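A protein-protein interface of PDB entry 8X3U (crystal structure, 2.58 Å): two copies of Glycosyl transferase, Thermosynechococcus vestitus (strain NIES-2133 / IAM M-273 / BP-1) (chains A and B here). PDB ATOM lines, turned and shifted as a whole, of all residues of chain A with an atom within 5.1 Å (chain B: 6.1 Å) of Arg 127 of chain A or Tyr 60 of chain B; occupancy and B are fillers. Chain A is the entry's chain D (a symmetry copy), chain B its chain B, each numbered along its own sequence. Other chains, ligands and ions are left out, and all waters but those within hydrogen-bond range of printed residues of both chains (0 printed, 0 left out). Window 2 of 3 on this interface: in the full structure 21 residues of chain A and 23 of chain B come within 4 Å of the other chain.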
ATOM      1  N   ALA A 123     -26.525  21.457   2.933  1.00  0.00           N
ATOM      2  CA  ALA A 123     -26.410  21.385   4.387  1.00  0.00           C
ATOM      3  C   ALA A 123     -25.387  22.390   4.908  1.00  0.00           C
ATOM      4  O   ALA A 123     -25.563  22.969   5.987  1.00  0.00           O
ATOM      5  CB  ALA A 123     -26.035  19.965   4.810  1.00  0.00           C
ATOM      6  N   ASP A 124     -24.307  22.606   4.152  1.00  0.00           N
ATOM      7  CA  ASP A 124     -23.276  23.558   4.548  1.00  0.00           C
ATOM      8  C   ASP A 124     -23.641  24.990   4.164  1.00  0.00           C
ATOM      9  O   ASP A 124     -23.625  25.884   5.017  1.00  0.00           O
ATOM     10  CB  ASP A 124     -21.929  23.157   3.943  1.00  0.00           C
ATOM     11  CG  ASP A 124     -21.269  22.010   4.693  1.00  0.00           C
ATOM     12  OD1 ASP A 124     -21.426  21.944   5.930  1.00  0.00           O
ATOM     13  OD2 ASP A 124     -20.592  21.177   4.051  1.00  0.00           O
ATOM     14  N   ASN A 125     -23.954  25.239   2.884  1.00  0.00           N
ATOM     15  CA  ASN A 125     -24.129  26.621   2.437  1.00  0.00           C
ATOM     16  C   ASN A 125     -25.324  27.306   3.093  1.00  0.00           C
ATOM     17  O   ASN A 125     -25.376  28.540   3.119  1.00  0.00           O
ATOM     18  CB  ASN A 125     -24.226  26.695   0.903  1.00  0.00           C
ATOM     19  CG  ASN A 125     -25.574  26.231   0.339  1.00  0.00           C
ATOM     20  OD1 ASN A 125     -26.529  25.944   1.063  1.00  0.00           O
ATOM     21  ND2 ASN A 125     -25.646  26.169  -0.985  1.00  0.00           N
ATOM     22  N   GLU A 126     -26.293  26.534   3.592  1.00  0.00           N
ATOM     23  CA  GLU A 126     -27.397  27.119   4.346  1.00  0.00           C
ATOM     24  C   GLU A 126     -26.895  27.975   5.502  1.00  0.00           C
ATOM     25  O   GLU A 126     -27.523  28.982   5.849  1.00  0.00           O
ATOM     26  CB  GLU A 126     -28.324  26.018   4.864  1.00  0.00           C
ATOM     27  CG  GLU A 126     -29.274  25.461   3.816  1.00  0.00           C
ATOM     28  CD  GLU A 126     -30.268  24.471   4.395  1.00  0.00           C
ATOM     29  OE1 GLU A 126     -30.252  24.260   5.626  1.00  0.00           O
ATOM     30  OE2 GLU A 126     -31.062  23.900   3.618  1.00  0.00           O
ATOM     31  N   ARG A 127     -25.762  27.601   6.102  1.00  0.00           N
ATOM     32  CA  ARG A 127     -25.299  28.293   7.298  1.00  0.00           C
ATOM     33  C   ARG A 127     -24.758  29.685   6.989  1.00  0.00           C
ATOM     34  O   ARG A 127     -24.935  30.600   7.799  1.00  0.00           O
ATOM     35  CB  ARG A 127     -24.223  27.459   7.995  1.00  0.00           C
ATOM     36  CG  ARG A 127     -24.491  25.959   8.005  1.00  0.00           C
ATOM     37  CD  ARG A 127     -25.255  25.516   9.244  1.00  0.00           C
ATOM     38  NE  ARG A 127     -24.358  25.186  10.350  1.00  0.00           N
ATOM     39  CZ  ARG A 127     -23.816  23.988  10.543  1.00  0.00           C
ATOM     40  NH1 ARG A 127     -24.070  22.998   9.697  1.00  0.00           N
ATOM     41  NH2 ARG A 127     -23.013  23.779  11.577  1.00  0.00           N
ATOM     42  N   ILE A 128     -24.116  29.875   5.834  1.00  0.00           N
ATOM     43  CA  ILE A 128     -23.626  31.208   5.490  1.00  0.00           C
ATOM     44  C   ILE A 128     -24.759  32.110   5.008  1.00  0.00           C
ATOM     45  O   ILE A 128     -24.759  33.317   5.279  1.00  0.00           O
ATOM     46  CB  ILE A 128     -22.488  31.121   4.454  1.00  0.00           C
ATOM     47  CG1 ILE A 128     -21.937  32.515   4.150  1.00  0.00           C
ATOM     48  CG2 ILE A 128     -22.964  30.473   3.165  1.00  0.00           C
ATOM     49  CD1 ILE A 128     -20.607  32.504   3.428  1.00  0.00           C
ATOM     50  N   PHE A 129     -25.745  31.553   4.300  1.00  0.00           N
ATOM     51  CA  PHE A 129     -26.883  32.364   3.869  1.00  0.00           C
ATOM     52  C   PHE A 129     -27.744  32.792   5.051  1.00  0.00           C
ATOM     53  O   PHE A 129     -28.211  33.937   5.099  1.00  0.00           O
ATOM     54  CB  PHE A 129     -27.713  31.598   2.840  1.00  0.00           C
ATOM     55  CG  PHE A 129     -27.069  31.521   1.484  1.00  0.00           C
ATOM     56  CD1 PHE A 129     -26.812  32.673   0.762  1.00  0.00           C
ATOM     57  CD2 PHE A 129     -26.720  30.299   0.934  1.00  0.00           C
ATOM     58  CE1 PHE A 129     -26.215  32.609  -0.483  1.00  0.00           C
ATOM     59  CE2 PHE A 129     -26.128  30.227  -0.311  1.00  0.00           C
ATOM     60  CZ  PHE A 129     -25.874  31.383  -1.020  1.00  0.00           C
ATOM     61  N   SER A 130     -27.968  31.885   6.005  1.00  0.00           N
ATOM     62  CA  SER A 130     -28.687  32.234   7.228  1.00  0.00           C
ATOM     63  C   SER A 130     -28.065  33.452   7.901  1.00  0.00           C
ATOM     64  O   SER A 130     -28.771  34.380   8.312  1.00  0.00           O
ATOM     65  CB  SER A 130     -28.701  31.042   8.184  1.00  0.00           C
ATOM     66  OG  SER A 130     -29.350  31.377   9.397  1.00  0.00           O
ATOM     67  N   GLN A 131     -26.738  33.448   8.038  1.00  0.00           N
ATOM     68  CA  GLN A 131     -26.030  34.548   8.683  1.00  0.00           C
ATOM     69  C   GLN A 131     -26.220  35.875   7.955  1.00  0.00           C
ATOM     70  O   GLN A 131     -26.098  36.935   8.580  1.00  0.00           O
ATOM     71  CB  GLN A 131     -24.539  34.201   8.770  1.00  0.00           C
ATOM     72  CG  GLN A 131     -23.682  35.160   9.590  1.00  0.00           C
ATOM     73  CD  GLN A 131     -24.133  35.273  11.033  1.00  0.00           C
ATOM     74  OE1 GLN A 131     -24.628  34.310  11.621  1.00  0.00           O
ATOM     75  NE2 GLN A 131     -23.957  36.454  11.616  1.00  0.00           N
ATOM     76  N   LEU B  12      -9.465  26.510   9.628  1.00  0.00           N
ATOM     77  CA  LEU B  12     -10.481  25.718  10.302  1.00  0.00           C
ATOM     78  C   LEU B  12     -10.339  24.226  10.050  1.00  0.00           C
ATOM     79  O   LEU B  12     -11.157  23.448  10.550  1.00  0.00           O
ATOM     80  CB  LEU B  12     -11.877  26.176   9.868  1.00  0.00           C
ATOM     81  CG  LEU B  12     -12.153  27.680   9.897  1.00  0.00           C
ATOM     82  CD1 LEU B  12     -13.591  27.952   9.487  1.00  0.00           C
ATOM     83  CD2 LEU B  12     -11.863  28.253  11.273  1.00  0.00           C
ATOM     84  N   ALA B  46     -11.168  30.607  15.477  1.00  0.00           N
ATOM     85  CA  ALA B  46     -10.771  29.242  15.191  1.00  0.00           C
ATOM     86  C   ALA B  46     -11.994  28.365  15.423  1.00  0.00           C
ATOM     87  O   ALA B  46     -13.066  28.849  15.789  1.00  0.00           O
ATOM     88  CB  ALA B  46      -9.569  28.829  16.053  1.00  0.00           C
ATOM     89  N   SER B  47     -11.827  27.071  15.178  1.00  0.00           N
ATOM     90  CA  SER B  47     -12.884  26.083  15.341  1.00  0.00           C
ATOM     91  C   SER B  47     -13.436  26.074  16.763  1.00  0.00           C
ATOM     92  O   SER B  47     -12.773  26.470  17.728  1.00  0.00           O
ATOM     93  CB  SER B  47     -12.357  24.701  14.981  1.00  0.00           C
ATOM     94  OG  SER B  47     -11.483  24.233  15.989  1.00  0.00           O
ATOM     95  N   GLY B  48     -14.679  25.598  16.878  1.00  0.00           N
ATOM     96  CA  GLY B  48     -15.403  25.642  18.135  1.00  0.00           C
ATOM     97  C   GLY B  48     -14.892  24.709  19.211  1.00  0.00           C
ATOM     98  O   GLY B  48     -15.152  24.952  20.393  1.00  0.00           O
ATOM     99  N   ASP B  49     -14.171  23.653  18.842  1.00  0.00           N
ATOM    100  CA  ASP B  49     -13.605  22.749  19.832  1.00  0.00           C
ATOM    101  C   ASP B  49     -12.180  23.126  20.215  1.00  0.00           C
ATOM    102  O   ASP B  49     -11.517  22.355  20.911  1.00  0.00           O
ATOM    103  CB  ASP B  49     -13.663  21.302  19.333  1.00  0.00           C
ATOM    104  CG  ASP B  49     -12.832  21.078  18.108  1.00  0.00           C
ATOM    105  OD1 ASP B  49     -12.545  22.078  17.418  1.00  0.00           O
ATOM    106  OD2 ASP B  49     -12.473  19.916  17.816  1.00  0.00           O
ATOM    107  N   SER B  58     -16.142  31.141  17.052  1.00  0.00           N
ATOM    108  CA  SER B  58     -16.099  30.030  16.112  1.00  0.00           C
ATOM    109  C   SER B  58     -17.325  30.036  15.211  1.00  0.00           C
ATOM    110  O   SER B  58     -18.435  30.339  15.655  1.00  0.00           O
ATOM    111  CB  SER B  58     -16.015  28.691  16.841  1.00  0.00           C
ATOM    112  OG  SER B  58     -17.264  28.332  17.406  1.00  0.00           O
ATOM    113  N   THR B  59     -17.114  29.692  13.943  1.00  0.00           N
ATOM    114  CA  THR B  59     -18.202  29.545  12.989  1.00  0.00           C
ATOM    115  C   THR B  59     -18.602  28.090  12.764  1.00  0.00           C
ATOM    116  O   THR B  59     -19.612  27.839  12.098  1.00  0.00           O
ATOM    117  CB  THR B  59     -17.823  30.191  11.648  1.00  0.00           C
ATOM    118  OG1 THR B  59     -16.643  29.572  11.125  1.00  0.00           O
ATOM    119  CG2 THR B  59     -17.559  31.678  11.838  1.00  0.00           C
ATOM    120  N   TYR B  60     -17.839  27.132  13.298  1.00  0.00           N
ATOM    121  CA  TYR B  60     -18.190  25.719  13.267  1.00  0.00           C
ATOM    122  C   TYR B  60     -17.625  25.042  14.507  1.00  0.00           C
ATOM    123  O   TYR B  60     -16.523  25.402  14.949  1.00  0.00           O
ATOM    124  CB  TYR B  60     -17.667  25.021  12.007  1.00  0.00           C
ATOM    125  CG  TYR B  60     -18.275  23.654  11.779  1.00  0.00           C
ATOM    126  CD1 TYR B  60     -19.575  23.520  11.304  1.00  0.00           C
ATOM    127  CD2 TYR B  60     -17.554  22.498  12.051  1.00  0.00           C
ATOM    128  CE1 TYR B  60     -20.136  22.273  11.100  1.00  0.00           C
ATOM    129  CE2 TYR B  60     -18.106  21.248  11.848  1.00  0.00           C
ATOM    130  CZ  TYR B  60     -19.397  21.141  11.377  1.00  0.00           C
ATOM    131  OH  TYR B  60     -19.949  19.897  11.171  1.00  0.00           O
ATOM    132  N   PRO B  61     -18.342  24.078  15.094  1.00  0.00           N
ATOM    133  CA  PRO B  61     -17.901  23.517  16.381  1.00  0.00           C
ATOM    134  C   PRO B  61     -16.722  22.556  16.291  1.00  0.00           C
ATOM    135  O   PRO B  61     -16.123  22.265  17.333  1.00  0.00           O
ATOM    136  CB  PRO B  61     -19.154  22.796  16.898  1.00  0.00           C
ATOM    137  CG  PRO B  61     -20.302  23.411  16.143  1.00  0.00           C
ATOM    138  CD  PRO B  61     -19.739  23.724  14.792  1.00  0.00           C
ATOM    139  N   HIS B  62     -16.362  22.054  15.111  1.00  0.00           N
ATOM    140  CA  HIS B  62     -15.381  20.980  15.030  1.00  0.00           C
ATOM    141  C   HIS B  62     -14.367  21.237  13.924  1.00  0.00           C
ATOM    142  O   HIS B  62     -14.597  22.026  13.004  1.00  0.00           O
ATOM    143  CB  HIS B  62     -16.053  19.625  14.789  1.00  0.00           C
ATOM    144  CG  HIS B  62     -17.017  19.229  15.865  1.00  0.00           C
ATOM    145  ND1 HIS B  62     -18.345  19.598  15.852  1.00  0.00           N
ATOM    146  CD2 HIS B  62     -16.842  18.498  16.990  1.00  0.00           C
ATOM    147  CE1 HIS B  62     -18.950  19.104  16.918  1.00  0.00           C
ATOM    148  NE2 HIS B  62     -18.059  18.432  17.626  1.00  0.00           N
ATOM    149  N   ALA B  63     -13.224  20.559  14.043  1.00  0.00           N
ATOM    150  CA  ALA B  63     -12.254  20.483  12.956  1.00  0.00           C
ATOM    151  C   ALA B  63     -12.914  19.957  11.696  1.00  0.00           C
ATOM    152  O   ALA B  63     -13.598  18.936  11.724  1.00  0.00           O
ATOM    153  CB  ALA B  63     -11.087  19.572  13.345  1.00  0.00           C
ATOM    154  N   ILE B  64     -12.644  20.616  10.572  1.00  0.00           N
ATOM    155  CA  ILE B  64     -13.393  20.307   9.360  1.00  0.00           C
ATOM    156  C   ILE B  64     -12.815  19.089   8.639  1.00  0.00           C
ATOM    157  O   ILE B  64     -13.564  18.318   8.026  1.00  0.00           O
ATOM    158  CB  ILE B  64     -13.431  21.558   8.465  1.00  0.00           C
ATOM    159  CG1 ILE B  64     -14.334  22.606   9.115  1.00  0.00           C
ATOM    160  CG2 ILE B  64     -13.900  21.232   7.061  1.00  0.00           C
ATOM    161  CD1 ILE B  64     -14.364  23.932   8.416  1.00  0.00           C
ATOM    162  N   ASP B  67     -14.318  16.007  10.229  1.00  0.00           N
ATOM    163  CA  ASP B  67     -15.745  16.103  10.515  1.00  0.00           C
ATOM    164  C   ASP B  67     -16.527  15.510   9.350  1.00  0.00           C
ATOM    165  O   ASP B  67     -16.356  15.959   8.211  1.00  0.00           O
ATOM    166  CB  ASP B  67     -16.142  17.553  10.737  1.00  0.00           C
ATOM    167  CG  ASP B  67     -17.477  17.695  11.419  1.00  0.00           C
ATOM    168  OD1 ASP B  67     -17.517  17.623  12.666  1.00  0.00           O
ATOM    169  OD2 ASP B  67     -18.487  17.885  10.709  1.00  0.00           O
ATOM    170  N   ASN B  69     -19.761  15.625   8.570  1.00  0.00           N
ATOM    171  CA  ASN B  69     -20.960  16.333   8.138  1.00  0.00           C
ATOM    172  C   ASN B  69     -20.682  17.522   7.227  1.00  0.00           C
ATOM    173  O   ASN B  69     -21.626  18.056   6.633  1.00  0.00           O
ATOM    174  CB  ASN B  69     -21.752  16.798   9.361  1.00  0.00           C
ATOM    175  CG  ASN B  69     -21.948  15.690  10.372  1.00  0.00           C
ATOM    176  OD1 ASN B  69     -22.080  14.520  10.008  1.00  0.00           O
ATOM    177  ND2 ASN B  69     -21.957  16.048  11.651  1.00  0.00           N
ATOM    178  N   VAL B  70     -19.429  17.952   7.095  1.00  0.00           N
ATOM    179  CA  VAL B  70     -19.076  19.140   6.325  1.00  0.00           C
ATOM    180  C   VAL B  70     -18.545  18.709   4.966  1.00  0.00           C
ATOM    181  O   VAL B  70     -17.700  17.807   4.875  1.00  0.00           O
ATOM    182  CB  VAL B  70     -18.046  20.004   7.073  1.00  0.00           C
ATOM    183  CG1 VAL B  70     -17.329  20.943   6.112  1.00  0.00           C
ATOM    184  CG2 VAL B  70     -18.725  20.795   8.162  1.00  0.00           C
ATOM    185  N   VAL B  75     -17.136  27.574   2.836  1.00  0.00           N
ATOM    186  CA  VAL B  75     -18.296  28.264   3.397  1.00  0.00           C
ATOM    187  C   VAL B  75     -17.953  28.852   4.759  1.00  0.00           C
ATOM    188  O   VAL B  75     -18.228  30.024   5.041  1.00  0.00           O
ATOM    189  CB  VAL B  75     -19.500  27.307   3.484  1.00  0.00           C
ATOM    190  CG1 VAL B  75     -20.618  27.933   4.295  1.00  0.00           C
ATOM    191  CG2 VAL B  75     -19.992  26.933   2.096  1.00  0.00           C
ATOM    192  N   TYR B  76     -17.334  28.044   5.619  1.00  0.00           N
ATOM    193  CA  TYR B  76     -17.038  28.473   6.980  1.00  0.00           C
ATOM    194  C   TYR B  76     -15.823  29.385   7.031  1.00  0.00           C
ATOM    195  O   TYR B  76     -15.727  30.237   7.921  1.00  0.00           O
ATOM    196  CB  TYR B  76     -16.858  27.243   7.871  1.00  0.00           C
ATOM    197  CG  TYR B  76     -18.056  26.326   7.796  1.00  0.00           C
ATOM    198  CD1 TYR B  76     -18.146  25.345   6.815  1.00  0.00           C
ATOM    199  CD2 TYR B  76     -19.114  26.466   8.682  1.00  0.00           C
ATOM    200  CE1 TYR B  76     -19.249  24.518   6.732  1.00  0.00           C
ATOM    201  CE2 TYR B  76     -20.221  25.641   8.607  1.00  0.00           C
ATOM    202  CZ  TYR B  76     -20.283  24.671   7.632  1.00  0.00           C
ATOM    203  OH  TYR B  76     -21.383  23.851   7.556  1.00  0.00           O
ATOM    204  N   LEU B  79     -17.413  32.647   6.431  1.00  0.00           N
ATOM    205  CA  LEU B  79     -18.028  33.053   7.691  1.00  0.00           C
ATOM    206  C   LEU B  79     -16.997  33.663   8.632  1.00  0.00           C
ATOM    207  O   LEU B  79     -17.259  34.684   9.280  1.00  0.00           O
ATOM    208  CB  LEU B  79     -18.731  31.862   8.341  1.00  0.00           C
ATOM    209  CG  LEU B  79     -20.113  31.512   7.779  1.00  0.00           C
ATOM    210  CD1 LEU B  79     -20.474  30.071   8.101  1.00  0.00           C
ATOM    211  CD2 LEU B  79     -21.167  32.462   8.317  1.00  0.00           C
ATOM    212  N   GLN B  80     -15.812  33.048   8.715  1.00  0.00           N
ATOM    213  CA  GLN B  80     -14.774  33.530   9.622  1.00  0.00           C
ATOM    214  C   GLN B  80     -14.314  34.930   9.239  1.00  0.00           C
ATOM    215  O   GLN B  80     -14.297  35.844  10.071  1.00  0.00           O
ATOM    216  CB  GLN B  80     -13.577  32.576   9.578  1.00  0.00           C
ATOM    217  CG  GLN B  80     -13.664  31.338  10.441  1.00  0.00           C
ATOM    218  CD  GLN B  80     -12.940  31.503  11.758  1.00  0.00           C
ATOM    219  OE1 GLN B  80     -11.831  32.031  11.802  1.00  0.00           O
ATOM    220  NE2 GLN B  80     -13.553  31.023  12.839  1.00  0.00           N
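No position is printed for both chains.
Of the 9 pairs that touch across the chains among the printed residues, none has its exchanged pair printed and touching as well.
OD1 of Asp 124 of chain A is in hydrogen-bond range of OH of Tyr 76 of chain B (2.5 Å).
Among the printed residues, pairs that only touch across the chains: Arg 127 of chain A with Tyr 60 of chain B (3.3 Å), Asp 124 of chain A with Val 70 of chain B (3.3 Å), Arg 127 of chain A with Tyr 76 of chain B (3.5 Å), Ile 128 of chain A with Val 75 of chain B (3.6 Å), Asp 124 of chain A with Val 75 of chain B (3.7 Å), Gln 131 of chain A with Leu 79 of chain B (3.8 Å), Ile 128 of chain A with Leu 79 of chain B (3.95 Å) and Asp 124 of chain A with Asn 69 of chain B (3.96 Å).
OD2 of Asp 67 of chain B sits close to N of Asn 69 of chain B (3.4 Å).
The side-chain hydroxyl of Tyr 60 of chain B is in hydrogen-bond range of the side-chain carboxylate of Asp 67 of chain B (2.5 Å).
OG1 of Thr 59 of chain B lies within hydrogen-bond range of O of Tyr 76 of chain B, 3.4 Å away.
O of Tyr 60 of chain B sits at hydrogen-bond distance from N of Gly 48 of chain B.
Of the 9 printed residues of chain A, 4 touch a printed residue of chain B.
Printed residues of chain A that touch a printed residue of chain B: Asp 124, Arg 127, Ile 128 and Gln 131.
Of the 19 printed residues of chain B, 6 touch a printed residue of chain A.
Printed residues of chain B that touch a printed residue of chain A: Tyr 60, Asn 69, Val 70, Val 75, Tyr 76 and Leu 79.
Of chain B, only Tyr 60 (3.3 Å) and Tyr 76 (3.5 Å) come within 4 Å of Arg 127 of chain A.
Printed residues of chain B within 4 Å of Gln 131 of chain A: Leu 79 (3.8 Å).
Ser 47 of chain B touches none of the printed residues of chain A.
Tyr 60 of chain B touches just one residue of chain A: Arg 127 (3.3 Å).
Of the printed residues of chain A, Asn 69 of chain B touches Asp 124 (3.96 Å).
Printed residues of chain A within 4 Å of Val 70 of chain B: Asp 124.
Of the printed residues of chain A, Val 75 of chain B touches Asp 124 (3.7 Å) and Ile 128 (3.6 Å).
Of the printed residues of chain A, Tyr 76 of chain B touches Asp 124 (2.5 Å) and Arg 127 (3.5 Å).
The nearest printed residue of chain B that does not touch Ile 128 of chain A is Tyr 76 of chain B (6.0 Å).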
